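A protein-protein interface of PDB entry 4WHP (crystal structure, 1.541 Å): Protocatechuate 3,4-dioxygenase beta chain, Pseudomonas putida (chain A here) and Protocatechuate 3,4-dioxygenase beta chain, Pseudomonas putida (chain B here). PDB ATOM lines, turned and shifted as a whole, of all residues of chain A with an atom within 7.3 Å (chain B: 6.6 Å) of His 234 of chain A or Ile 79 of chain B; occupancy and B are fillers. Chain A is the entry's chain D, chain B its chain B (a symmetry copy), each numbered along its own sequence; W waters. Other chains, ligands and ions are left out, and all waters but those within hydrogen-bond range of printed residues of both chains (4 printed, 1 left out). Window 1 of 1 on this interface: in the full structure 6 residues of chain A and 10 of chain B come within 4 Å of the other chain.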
ATOM      1  N   ARG A   7      -3.479  24.742   0.981  1.00  0.00           N
ATOM      2  CA  ARG A   7      -4.058  23.450   0.679  1.00  0.00           C
ATOM      3  C   ARG A   7      -4.888  23.010   1.877  1.00  0.00           C
ATOM      4  O   ARG A   7      -4.599  23.385   3.014  1.00  0.00           O
ATOM      5  CB  ARG A   7      -2.970  22.423   0.368  1.00  0.00           C
ATOM      6  CG  ARG A   7      -2.133  22.778  -0.847  1.00  0.00           C
ATOM      7  CD  ARG A   7      -2.902  22.586  -2.130  1.00  0.00           C
ATOM      8  NE  ARG A   7      -2.192  23.081  -3.311  1.00  0.00           N
ATOM      9  CZ  ARG A   7      -2.474  24.215  -3.944  1.00  0.00           C
ATOM     10  NH1 ARG A   7      -3.452  24.996  -3.506  1.00  0.00           N
ATOM     11  NH2 ARG A   7      -1.784  24.554  -5.038  1.00  0.00           N
ATOM     12  N   ARG A 231      -3.061  24.236   5.289  1.00  0.00           N
ATOM     13  CA  ARG A 231      -1.605  24.360   5.305  1.00  0.00           C
ATOM     14  C   ARG A 231      -1.098  25.148   4.105  1.00  0.00           C
ATOM     15  O   ARG A 231      -1.802  25.324   3.108  1.00  0.00           O
ATOM     16  CB  ARG A 231      -0.965  22.973   5.319  1.00  0.00           C
ATOM     17  CG  ARG A 231      -1.115  22.195   4.029  1.00  0.00           C
ATOM     18  CD  ARG A 231      -0.193  20.978   4.022  1.00  0.00           C
ATOM     19  NE  ARG A 231      -0.435  20.070   2.905  1.00  0.00           N
ATOM     20  CZ  ARG A 231      -0.023  20.256   1.652  1.00  0.00           C
ATOM     21  NH1 ARG A 231       0.627  21.354   1.298  1.00  0.00           N
ATOM     22  NH2 ARG A 231      -0.303  19.339   0.728  1.00  0.00           N
ATOM     23  N   LYS A 232       0.139  25.616   4.212  1.00  0.00           N
ATOM     24  CA  LYS A 232       0.809  26.240   3.092  1.00  0.00           C
ATOM     25  C   LYS A 232       1.146  25.187   2.053  1.00  0.00           C
ATOM     26  O   LYS A 232       1.319  24.007   2.374  1.00  0.00           O
ATOM     27  CB  LYS A 232       2.102  26.938   3.546  1.00  0.00           C
ATOM     28  CG  LYS A 232       1.866  28.180   4.384  1.00  0.00           C
ATOM     29  CD  LYS A 232       3.165  28.900   4.710  1.00  0.00           C
ATOM     30  CE  LYS A 232       2.900  30.179   5.489  1.00  0.00           C
ATOM     31  NZ  LYS A 232       4.147  30.959   5.715  1.00  0.00           N
ATOM     32  N   THR A 233       1.260  25.627   0.806  1.00  0.00           N
ATOM     33  CA  THR A 233       1.789  24.775  -0.249  1.00  0.00           C
ATOM     34  C   THR A 233       3.262  24.485   0.022  1.00  0.00           C
ATOM     35  O   THR A 233       3.966  25.275   0.664  1.00  0.00           O
ATOM     36  CB  THR A 233       1.672  25.439  -1.622  1.00  0.00           C
ATOM     37  OG1 THR A 233       2.339  26.699  -1.595  1.00  0.00           O
ATOM     38  CG2 THR A 233       0.229  25.648  -1.994  1.00  0.00           C
ATOM     39  N   HIS A 234       3.723  23.331  -0.455  1.00  0.00           N
ATOM     40  CA  HIS A 234       5.129  22.984  -0.320  1.00  0.00           C
ATOM     41  C   HIS A 234       5.573  22.056  -1.434  1.00  0.00           C
ATOM     42  O   HIS A 234       4.877  21.108  -1.767  1.00  0.00           O
ATOM     43  CB  HIS A 234       5.464  22.399   1.069  1.00  0.00           C
ATOM     44  CG  HIS A 234       4.574  21.280   1.534  1.00  0.00           C
ATOM     45  ND1 HIS A 234       4.045  20.319   0.698  1.00  0.00           N
ATOM     46  CD2 HIS A 234       4.165  20.951   2.783  1.00  0.00           C
ATOM     47  CE1 HIS A 234       3.330  19.461   1.407  1.00  0.00           C
ATOM     48  NE2 HIS A 234       3.397  19.816   2.676  1.00  0.00           N
ATOM     49  N   PHE A 235       6.744  22.343  -1.997  1.00  0.00           N
ATOM     50  CA  PHE A 235       7.358  21.496  -3.014  1.00  0.00           C
ATOM     51  C   PHE A 235       6.442  21.190  -4.204  1.00  0.00           C
ATOM     52  O   PHE A 235       6.460  20.081  -4.740  1.00  0.00           O
ATOM     53  CB  PHE A 235       7.870  20.181  -2.406  1.00  0.00           C
ATOM     54  CG  PHE A 235       8.833  20.368  -1.266  1.00  0.00           C
ATOM     55  CD1 PHE A 235      10.142  20.754  -1.503  1.00  0.00           C
ATOM     56  CD2 PHE A 235       8.436  20.150   0.037  1.00  0.00           C
ATOM     57  CE1 PHE A 235      11.039  20.924  -0.466  1.00  0.00           C
ATOM     58  CE2 PHE A 235       9.332  20.302   1.086  1.00  0.00           C
ATOM     59  CZ  PHE A 235      10.633  20.703   0.834  1.00  0.00           C
ATOM     60  N   GLU A 236       5.649  22.171  -4.624  1.00  0.00           N
ATOM     61  CA  GLU A 236       4.806  21.991  -5.812  1.00  0.00           C
ATOM     62  C   GLU A 236       5.494  22.487  -7.075  1.00  0.00           C
ATOM     63  O   GLU A 236       6.241  23.464  -7.037  1.00  0.00           O
ATOM     64  CB  GLU A 236       3.462  22.692  -5.640  1.00  0.00           C
ATOM     65  CG  GLU A 236       2.616  22.041  -4.565  1.00  0.00           C
ATOM     66  CD  GLU A 236       1.156  22.437  -4.611  1.00  0.00           C
ATOM     67  OE1 GLU A 236       0.731  23.171  -5.538  1.00  0.00           O
ATOM     68  OE2 GLU A 236       0.427  21.990  -3.700  1.00  0.00           O
ATOM     69  N   ASN A 237       5.253  21.782  -8.180  1.00  0.00           N
ATOM     70  CA  ASN A 237       5.805  22.153  -9.493  1.00  0.00           C
ATOM     71  C   ASN A 237       7.332  22.146  -9.492  1.00  0.00           C
ATOM     72  O   ASN A 237       7.973  23.020 -10.081  1.00  0.00           O
ATOM     73  CB  ASN A 237       5.285  23.526  -9.944  1.00  0.00           C
ATOM     74  CG  ASN A 237       3.772  23.615  -9.922  1.00  0.00           C
ATOM     75  OD1 ASN A 237       3.079  22.695 -10.369  1.00  0.00           O
ATOM     76  ND2 ASN A 237       3.247  24.719  -9.392  1.00  0.00           N
ATOM     77  N   CYS A 238       7.896  21.147  -8.820  1.00  0.00           N
ATOM     78  CA  CYS A 238       9.346  20.963  -8.702  1.00  0.00           C
ATOM     79  C   CYS A 238       9.624  19.538  -8.210  1.00  0.00           C
ATOM     80  O   CYS A 238      10.733  19.005  -8.379  1.00  0.00           O
ATOM     81  CB  CYS A 238       9.985  22.007  -7.752  1.00  0.00           C
ATOM     82  SG  CYS A 238       9.624  21.866  -5.967  1.00  0.00           S
ATOM     83  N   ARG B  77       9.371   9.041  -2.892  1.00  0.00           N
ATOM     84  CA  ARG B  77       9.372  10.491  -2.670  1.00  0.00           C
ATOM     85  C   ARG B  77       8.659  10.811  -1.372  1.00  0.00           C
ATOM     86  O   ARG B  77       7.487  10.472  -1.212  1.00  0.00           O
ATOM     87  CB  ARG B  77       8.676  11.217  -3.824  1.00  0.00           C
ATOM     88  CG  ARG B  77       9.338  11.018  -5.172  1.00  0.00           C
ATOM     89  CD  ARG B  77       8.411  11.427  -6.303  1.00  0.00           C
ATOM     90  NE  ARG B  77       8.016  12.836  -6.294  1.00  0.00           N
ATOM     91  CZ  ARG B  77       8.671  13.826  -6.902  1.00  0.00           C
ATOM     92  NH1 ARG B  77       9.804  13.594  -7.560  1.00  0.00           N
ATOM     93  NH2 ARG B  77       8.187  15.053  -6.849  1.00  0.00           N
ATOM     94  N   ILE B  78       9.360  11.465  -0.454  1.00  0.00           N
ATOM     95  CA  ILE B  78       8.775  11.864   0.833  1.00  0.00           C
ATOM     96  C   ILE B  78       9.199  13.253   1.259  1.00  0.00           C
ATOM     97  O   ILE B  78      10.329  13.687   1.007  1.00  0.00           O
ATOM     98  CB  ILE B  78       9.110  10.869   1.979  1.00  0.00           C
ATOM     99  CG1 ILE B  78      10.628  10.701   2.170  1.00  0.00           C
ATOM    100  CG2 ILE B  78       8.463   9.520   1.702  1.00  0.00           C
ATOM    101  CD1 ILE B  78      10.991   9.906   3.405  1.00  0.00           C
ATOM    102  N   ILE B  79       8.287  13.912   1.963  1.00  0.00           N
ATOM    103  CA  ILE B  79       8.591  15.053   2.790  1.00  0.00           C
ATOM    104  C   ILE B  79       8.848  14.551   4.219  1.00  0.00           C
ATOM    105  O   ILE B  79       8.124  13.686   4.730  1.00  0.00           O
ATOM    106  CB  ILE B  79       7.437  16.074   2.759  1.00  0.00           C
ATOM    107  CG1 ILE B  79       7.346  16.694   1.356  1.00  0.00           C
ATOM    108  CG2 ILE B  79       7.623  17.134   3.835  1.00  0.00           C
ATOM    109  CD1 ILE B  79       6.064  17.452   1.109  1.00  0.00           C
ATOM    110  N   VAL B  80       9.894  15.073   4.848  1.00  0.00           N
ATOM    111  CA  VAL B  80      10.145  14.839   6.274  1.00  0.00           C
ATOM    112  C   VAL B  80      10.072  16.206   6.943  1.00  0.00           C
ATOM    113  O   VAL B  80      10.831  17.101   6.611  1.00  0.00           O
ATOM    114  CB  VAL B  80      11.505  14.167   6.534  1.00  0.00           C
ATOM    115  CG1 VAL B  80      11.718  13.961   8.034  1.00  0.00           C
ATOM    116  CG2 VAL B  80      11.601  12.843   5.796  1.00  0.00           C
ATOM    117  N   ALA B  81       9.147  16.359   7.872  1.00  0.00           N
ATOM    118  CA  ALA B  81       8.862  17.639   8.494  1.00  0.00           C
ATOM    119  C   ALA B  81       8.561  17.428   9.960  1.00  0.00           C
ATOM    120  O   ALA B  81       8.201  16.332  10.386  1.00  0.00           O
ATOM    121  CB  ALA B  81       7.674  18.304   7.817  1.00  0.00           C
ATOM    122  N   TYR B 137      10.539  22.668  10.606  1.00  0.00           N
ATOM    123  CA  TYR B 137      11.516  22.383   9.551  1.00  0.00           C
ATOM    124  C   TYR B 137      10.858  21.495   8.479  1.00  0.00           C
ATOM    125  O   TYR B 137       9.828  20.833   8.721  1.00  0.00           O
ATOM    126  CB  TYR B 137      12.772  21.712  10.122  1.00  0.00           C
ATOM    127  CG  TYR B 137      12.541  20.279  10.512  1.00  0.00           C
ATOM    128  CD1 TYR B 137      12.695  19.267   9.583  1.00  0.00           C
ATOM    129  CD2 TYR B 137      12.155  19.927  11.809  1.00  0.00           C
ATOM    130  CE1 TYR B 137      12.451  17.952   9.913  1.00  0.00           C
ATOM    131  CE2 TYR B 137      11.906  18.613  12.140  1.00  0.00           C
ATOM    132  CZ  TYR B 137      12.069  17.627  11.194  1.00  0.00           C
ATOM    133  OH  TYR B 137      11.803  16.313  11.503  1.00  0.00           O
ATOM    134  N   SER B 138      11.469  21.450   7.302  1.00  0.00           N
ATOM    135  CA  SER B 138      10.991  20.616   6.215  1.00  0.00           C
ATOM    136  C   SER B 138      12.139  20.240   5.282  1.00  0.00           C
ATOM    137  O   SER B 138      12.929  21.100   4.876  1.00  0.00           O
ATOM    138  CB  SER B 138       9.914  21.390   5.444  1.00  0.00           C
ATOM    139  OG  SER B 138       9.402  20.649   4.377  1.00  0.00           O
ATOM    140  N   PHE B 139      12.205  18.957   4.946  1.00  0.00           N
ATOM    141  CA  PHE B 139      13.052  18.425   3.882  1.00  0.00           C
ATOM    142  C   PHE B 139      12.206  17.646   2.872  1.00  0.00           C
ATOM    143  O   PHE B 139      11.135  17.128   3.213  1.00  0.00           O
ATOM    144  CB  PHE B 139      14.070  17.438   4.439  1.00  0.00           C
ATOM    145  CG  PHE B 139      15.028  18.022   5.426  1.00  0.00           C
ATOM    146  CD1 PHE B 139      16.111  18.761   4.990  1.00  0.00           C
ATOM    147  CD2 PHE B 139      14.868  17.824   6.784  1.00  0.00           C
ATOM    148  CE1 PHE B 139      17.004  19.293   5.893  1.00  0.00           C
ATOM    149  CE2 PHE B 139      15.774  18.335   7.698  1.00  0.00           C
ATOM    150  CZ  PHE B 139      16.852  19.079   7.249  1.00  0.00           C
ATOM    151  N   ARG B 140      12.705  17.534   1.646  1.00  0.00           N
ATOM    152  CA  ARG B 140      12.170  16.595   0.679  1.00  0.00           C
ATOM    153  C   ARG B 140      13.286  15.638   0.296  1.00  0.00           C
ATOM    154  O   ARG B 140      14.427  16.041   0.096  1.00  0.00           O
ATOM    155  CB  ARG B 140      11.607  17.310  -0.551  1.00  0.00           C
ATOM    156  CG  ARG B 140      10.884  16.355  -1.497  1.00  0.00           C
ATOM    157  CD  ARG B 140      10.172  17.042  -2.647  1.00  0.00           C
ATOM    158  NE  ARG B 140      11.110  17.687  -3.560  1.00  0.00           N
ATOM    159  CZ  ARG B 140      10.804  18.072  -4.801  1.00  0.00           C
ATOM    160  NH1 ARG B 140      11.732  18.663  -5.543  1.00  0.00           N
ATOM    161  NH2 ARG B 140       9.581  17.878  -5.286  1.00  0.00           N
ATOM    162  N   THR B 141      12.957  14.352   0.249  1.00  0.00           N
ATOM    163  CA  THR B 141      13.956  13.327   0.025  1.00  0.00           C
ATOM    164  C   THR B 141      13.328  12.049  -0.536  1.00  0.00           C
ATOM    165  O   THR B 141      12.170  12.047  -0.971  1.00  0.00           O
ATOM    166  CB  THR B 141      14.747  13.076   1.326  1.00  0.00           C
ATOM    167  OG1 THR B 141      15.892  12.258   1.071  1.00  0.00           O
ATOM    168  CG2 THR B 141      13.881  12.449   2.412  1.00  0.00           C
ATOM    169  N   ASN B 211      -1.749  13.996   5.958  1.00  0.00           N
ATOM    170  CA  ASN B 211      -2.197  15.376   5.941  1.00  0.00           C
ATOM    171  C   ASN B 211      -1.216  16.320   5.266  1.00  0.00           C
ATOM    172  O   ASN B 211      -1.615  17.348   4.717  1.00  0.00           O
ATOM    173  CB  ASN B 211      -2.476  15.864   7.377  1.00  0.00           C
ATOM    174  CG  ASN B 211      -3.131  14.804   8.240  1.00  0.00           C
ATOM    175  OD1 ASN B 211      -4.319  14.530   8.107  1.00  0.00           O
ATOM    176  ND2 ASN B 211      -2.347  14.186   9.121  1.00  0.00           N
ATOM    177  N   ASN B 212       0.070  15.977   5.327  1.00  0.00           N
ATOM    178  CA  ASN B 212       1.130  16.815   4.784  1.00  0.00           C
ATOM    179  C   ASN B 212       1.653  16.328   3.420  1.00  0.00           C
ATOM    180  O   ASN B 212       2.564  16.933   2.854  1.00  0.00           O
ATOM    181  CB  ASN B 212       2.279  16.870   5.782  1.00  0.00           C
ATOM    182  CG  ASN B 212       3.089  18.135   5.671  1.00  0.00           C
ATOM    183  OD1 ASN B 212       2.570  19.185   5.272  1.00  0.00           O
ATOM    184  ND2 ASN B 212       4.381  18.049   6.011  1.00  0.00           N
ATOM    185  N   ALA B 213       1.095  15.231   2.908  1.00  0.00           N
ATOM    186  CA  ALA B 213       1.462  14.723   1.595  1.00  0.00           C
ATOM    187  C   ALA B 213       1.025  15.654   0.477  1.00  0.00           C
ATOM    188  O   ALA B 213       0.046  16.415   0.621  1.00  0.00           O
ATOM    189  CB  ALA B 213       0.859  13.342   1.373  1.00  0.00           C
ATOM    190  N   ASN B 214       1.764  15.593  -0.638  1.00  0.00           N
ATOM    191  CA  ASN B 214       1.314  16.192  -1.894  1.00  0.00           C
ATOM    192  C   ASN B 214       0.659  15.100  -2.711  1.00  0.00           C
ATOM    193  O   ASN B 214       1.346  14.201  -3.191  1.00  0.00           O
ATOM    194  CB  ASN B 214       2.478  16.737  -2.734  1.00  0.00           C
ATOM    195  CG  ASN B 214       2.997  18.078  -2.268  1.00  0.00           C
ATOM    196  OD1 ASN B 214       2.441  18.729  -1.385  1.00  0.00           O
ATOM    197  ND2 ASN B 214       4.080  18.520  -2.906  1.00  0.00           N
ATOM    198  N   ASP B 217       2.054  12.830  -5.838  1.00  0.00           N
ATOM    199  CA  ASP B 217       3.412  13.370  -5.889  1.00  0.00           C
ATOM    200  C   ASP B 217       4.324  12.734  -4.830  1.00  0.00           C
ATOM    201  O   ASP B 217       5.188  11.920  -5.155  1.00  0.00           O
ATOM    202  CB  ASP B 217       3.316  14.901  -5.780  1.00  0.00           C
ATOM    203  CG  ASP B 217       4.644  15.605  -5.646  1.00  0.00           C
ATOM    204  OD1 ASP B 217       5.700  14.941  -5.581  1.00  0.00           O
ATOM    205  OD2 ASP B 217       4.596  16.868  -5.601  1.00  0.00           O
ATOM    206  N   CYS B 218       4.115  13.065  -3.568  1.00  0.00           N
ATOM    207  CA  CYS B 218       4.971  12.554  -2.516  1.00  0.00           C
ATOM    208  C   CYS B 218       4.215  12.343  -1.215  1.00  0.00           C
ATOM    209  O   CYS B 218       3.262  13.061  -0.896  1.00  0.00           O
ATOM    210  CB  CYS B 218       6.138  13.488  -2.273  1.00  0.00           C
ATOM    211  SG  CYS B 218       5.709  15.096  -1.595  1.00  0.00           S
ATOM    212  N   LEU B 219       4.651  11.337  -0.469  1.00  0.00           N
ATOM    213  CA  LEU B 219       4.136  11.104   0.882  1.00  0.00           C
ATOM    214  C   LEU B 219       4.863  12.018   1.875  1.00  0.00           C
ATOM    215  O   LEU B 219       5.687  12.854   1.480  1.00  0.00           O
ATOM    216  CB  LEU B 219       4.243   9.609   1.246  1.00  0.00           C
ATOM    217  CG  LEU B 219       3.103   8.786   0.648  1.00  0.00           C
ATOM    218  CD1 LEU B 219       3.420   7.309   0.767  1.00  0.00           C
ATOM    219  CD2 LEU B 219       1.774   9.079   1.313  1.00  0.00           C
ATOM    220  N   ALA B 220       4.517  11.908   3.154  1.00  0.00           N
ATOM    221  CA  ALA B 220       5.140  12.726   4.191  1.00  0.00           C
ATOM    222  C   ALA B 220       5.222  11.961   5.489  1.00  0.00           C
ATOM    223  O   ALA B 220       4.354  11.132   5.793  1.00  0.00           O
ATOM    224  CB  ALA B 220       4.366  14.027   4.387  1.00  0.00           C
ATOM    225  N   TYR B 221       6.295  12.232   6.219  1.00  0.00           N
ATOM    226  CA  TYR B 221       6.504  11.734   7.569  1.00  0.00           C
ATOM    227  C   TYR B 221       6.712  12.914   8.502  1.00  0.00           C
ATOM    228  O   TYR B 221       7.244  13.951   8.101  1.00  0.00           O
ATOM    229  CB  TYR B 221       7.708  10.779   7.603  1.00  0.00           C
ATOM    230  CG  TYR B 221       7.326   9.407   7.103  1.00  0.00           C
ATOM    231  CD1 TYR B 221       7.337   9.098   5.749  1.00  0.00           C
ATOM    232  CD2 TYR B 221       6.918   8.421   7.990  1.00  0.00           C
ATOM    233  CE1 TYR B 221       6.946   7.837   5.295  1.00  0.00           C
ATOM    234  CE2 TYR B 221       6.537   7.172   7.557  1.00  0.00           C
ATOM    235  CZ  TYR B 221       6.536   6.879   6.213  1.00  0.00           C
ATOM    236  OH  TYR B 221       6.140   5.610   5.809  1.00  0.00           O
ATOM    237  N   ARG B 222       6.299  12.735   9.752  1.00  0.00           N
ATOM    238  CA  ARG B 222       6.429  13.757  10.787  1.00  0.00           C
ATOM    239  C   ARG B 222       7.365  13.292  11.888  1.00  0.00           C
ATOM    240  O   ARG B 222       7.173  12.223  12.447  1.00  0.00           O
ATOM    241  CB  ARG B 222       5.072  14.150  11.387  1.00  0.00           C
ATOM    242  CG  ARG B 222       5.181  15.360  12.321  1.00  0.00           C
ATOM    243  CD  ARG B 222       3.911  16.174  12.401  1.00  0.00           C
ATOM    244  NE  ARG B 222       3.543  16.736  11.119  1.00  0.00           N
ATOM    245  CZ  ARG B 222       3.886  17.950  10.679  1.00  0.00           C
ATOM    246  NH1 ARG B 222       3.480  18.333   9.479  1.00  0.00           N
ATOM    247  NH2 ARG B 222       4.600  18.795  11.418  1.00  0.00           N
HETATM  248  O   HOH W   1       1.683  21.389  -1.354  1.00  0.00           O
HETATM  249  O   HOH W   2      10.085  16.258  -8.771  1.00  0.00           O
HETATM  250  O   HOH W   3       7.067  17.292  -4.204  1.00  0.00           O
HETATM  251  O   HOH W   4       6.328  18.041  -7.518  1.00  0.00           O
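The backbone carbonyl oxygen of His 234 of chain A is in hydrogen-bond range of the side-chain amide nitrogen of Asn 214 of chain B (2.9 Å).
The backbone carbonyl oxygen (O) of Cys 238 of chain A lies within hydrogen-bond range of the guanidinium group (NH1) of Arg 140 of chain B (3.0 Å).
The guanidinium group (NH2) of Arg 231 of chain A is in hydrogen-bond range of the backbone carbonyl oxygen (O) of Ala 213 of chain B.
The side-chain amide nitrogen (ND2) of Asn 214 of chain B is in hydrogen-bond range of the backbone carbonyl oxygen (O) of Phe 235 of chain A, 3.4 Å away.
The backbone carbonyl oxygen (O) of Asn 211 of chain B lies within hydrogen-bond range of the guanidinium group (NE) of Arg 231 of chain A (3.5 Å).
The side-chain amide oxygen (OD1) of Asn 212 of chain B is in hydrogen-bond range of a ring nitrogen (NE2) of His 234 of chain A (2.8 Å).
Among the printed residues, merely in contact across the chains: Phe 235 of chain A with Ser 138 of chain B (3.3 Å), His 234 of chain A with Ile 79 of chain B (3.4 Å), Arg 231 of chain A with Asn 214 of chain B (3.5 Å), Arg 231 of chain A with Asn 212 of chain B (3.5 Å), Phe 235 of chain A with Arg 140 of chain B (3.7 Å), Phe 235 of chain A with Ile 79 of chain B (3.7 Å), Phe 235 of chain A with Asp 217 of chain B (3.8 Å) and Phe 235 of chain A with Phe 139 of chain B (3.997 Å).
Water W1 lies within hydrogen-bond range of OE2 of Glu 236 of chain A (2.7 Å), OD1 of Asn 214 of chain B (2.8 Å), NH1 of Arg 231 of chain A (2.9 Å) and N of His 234 of chain A (3.0 Å).
Water W3 lies within hydrogen-bond range of the guanidinium group of Arg 140 of chain B (2.8 Å), the side-chain carboxylate of Asp 217 of chain B (2.9 Å), the backbone carbonyl oxygen of Phe 235 of chain A (2.9 Å), the side-chain amide nitrogen of Asn 214 of chain B (3.5 Å) and the side-chain sulfur of Cys 218 of chain B (3.7 Å).
Water W4 lies within hydrogen-bond range of OD2 of Asp 217 of chain B (2.8 Å) and O of Phe 235 of chain A (3.4 Å).
Water W2 lies within hydrogen-bond range of the backbone carbonyl oxygen (O) of Cys 238 of chain A (2.8 Å) and the guanidinium group (NH1) of Arg 77 of chain B (2.9 Å).
Of the 20 printed residues of chain B, 9 touch a printed residue of chain A.
Hydrophobic or aromatic side chains of chain B that line the printed part of chain A: Ile 79.
Along chain B the printed residues that touch a printed residue of chain A span positions 79 to 217.
Printed residues of chain A that touch a printed residue of chain B: Arg 231, His 234, Phe 235 and Cys 238.
Hydrophobic or aromatic side chains of chain A that line the printed part of chain B: His 234 and Phe 235.
Among the printed residues, 14 pairs touch across the chains.
Among the printed residues, no Asp or Glu carboxylate lies within 4 Å of a Lys or Arg side-chain nitrogen of the other chain.
His 234 of chain A touches three residues of chain B.
Ile 79 of chain B touches just these residues of chain A: His 234 and Phe 235.
Printed residues of chain A within 4 Å of Phe 139 of chain B: Phe 235.
Of the printed residues of chain B, Arg 231 of chain A touches Asn 211 (3.5 Å), Asn 212 (3.5 Å), Ala 213 (2.9 Å) and Asn 214 (3.5 Å).
The backbone carbonyl oxygen (O) of Val 80 of chain B sits at hydrogen-bond distance from the backbone NH (N) of Phe 139 of chain B, 2.8 Å away.
A ring nitrogen (NE2) of His 234 of chain A lies close to the guanidinium group (NH1) of Arg 231 of chain A, at 3.5 Å.
The backbone carbonyl oxygen of Arg 231 of chain A lies within hydrogen-bond range of the backbone NH of Arg 7 of chain A, 2.8 Å away.
The guanidinium group (NH2) of Arg 77 of chain B lies within salt-bridge range of the side-chain carboxylate (OD1) of Asp 217 of chain B.
ND2 of Asn 214 of chain B sits at hydrogen-bond distance from OD2 of Asp 217 of chain B (3.2 Å).
The backbone NH (N) of Ile 79 of chain B is in hydrogen-bond range of the backbone carbonyl oxygen (O) of Leu 219 of chain B, at 2.8 Å.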
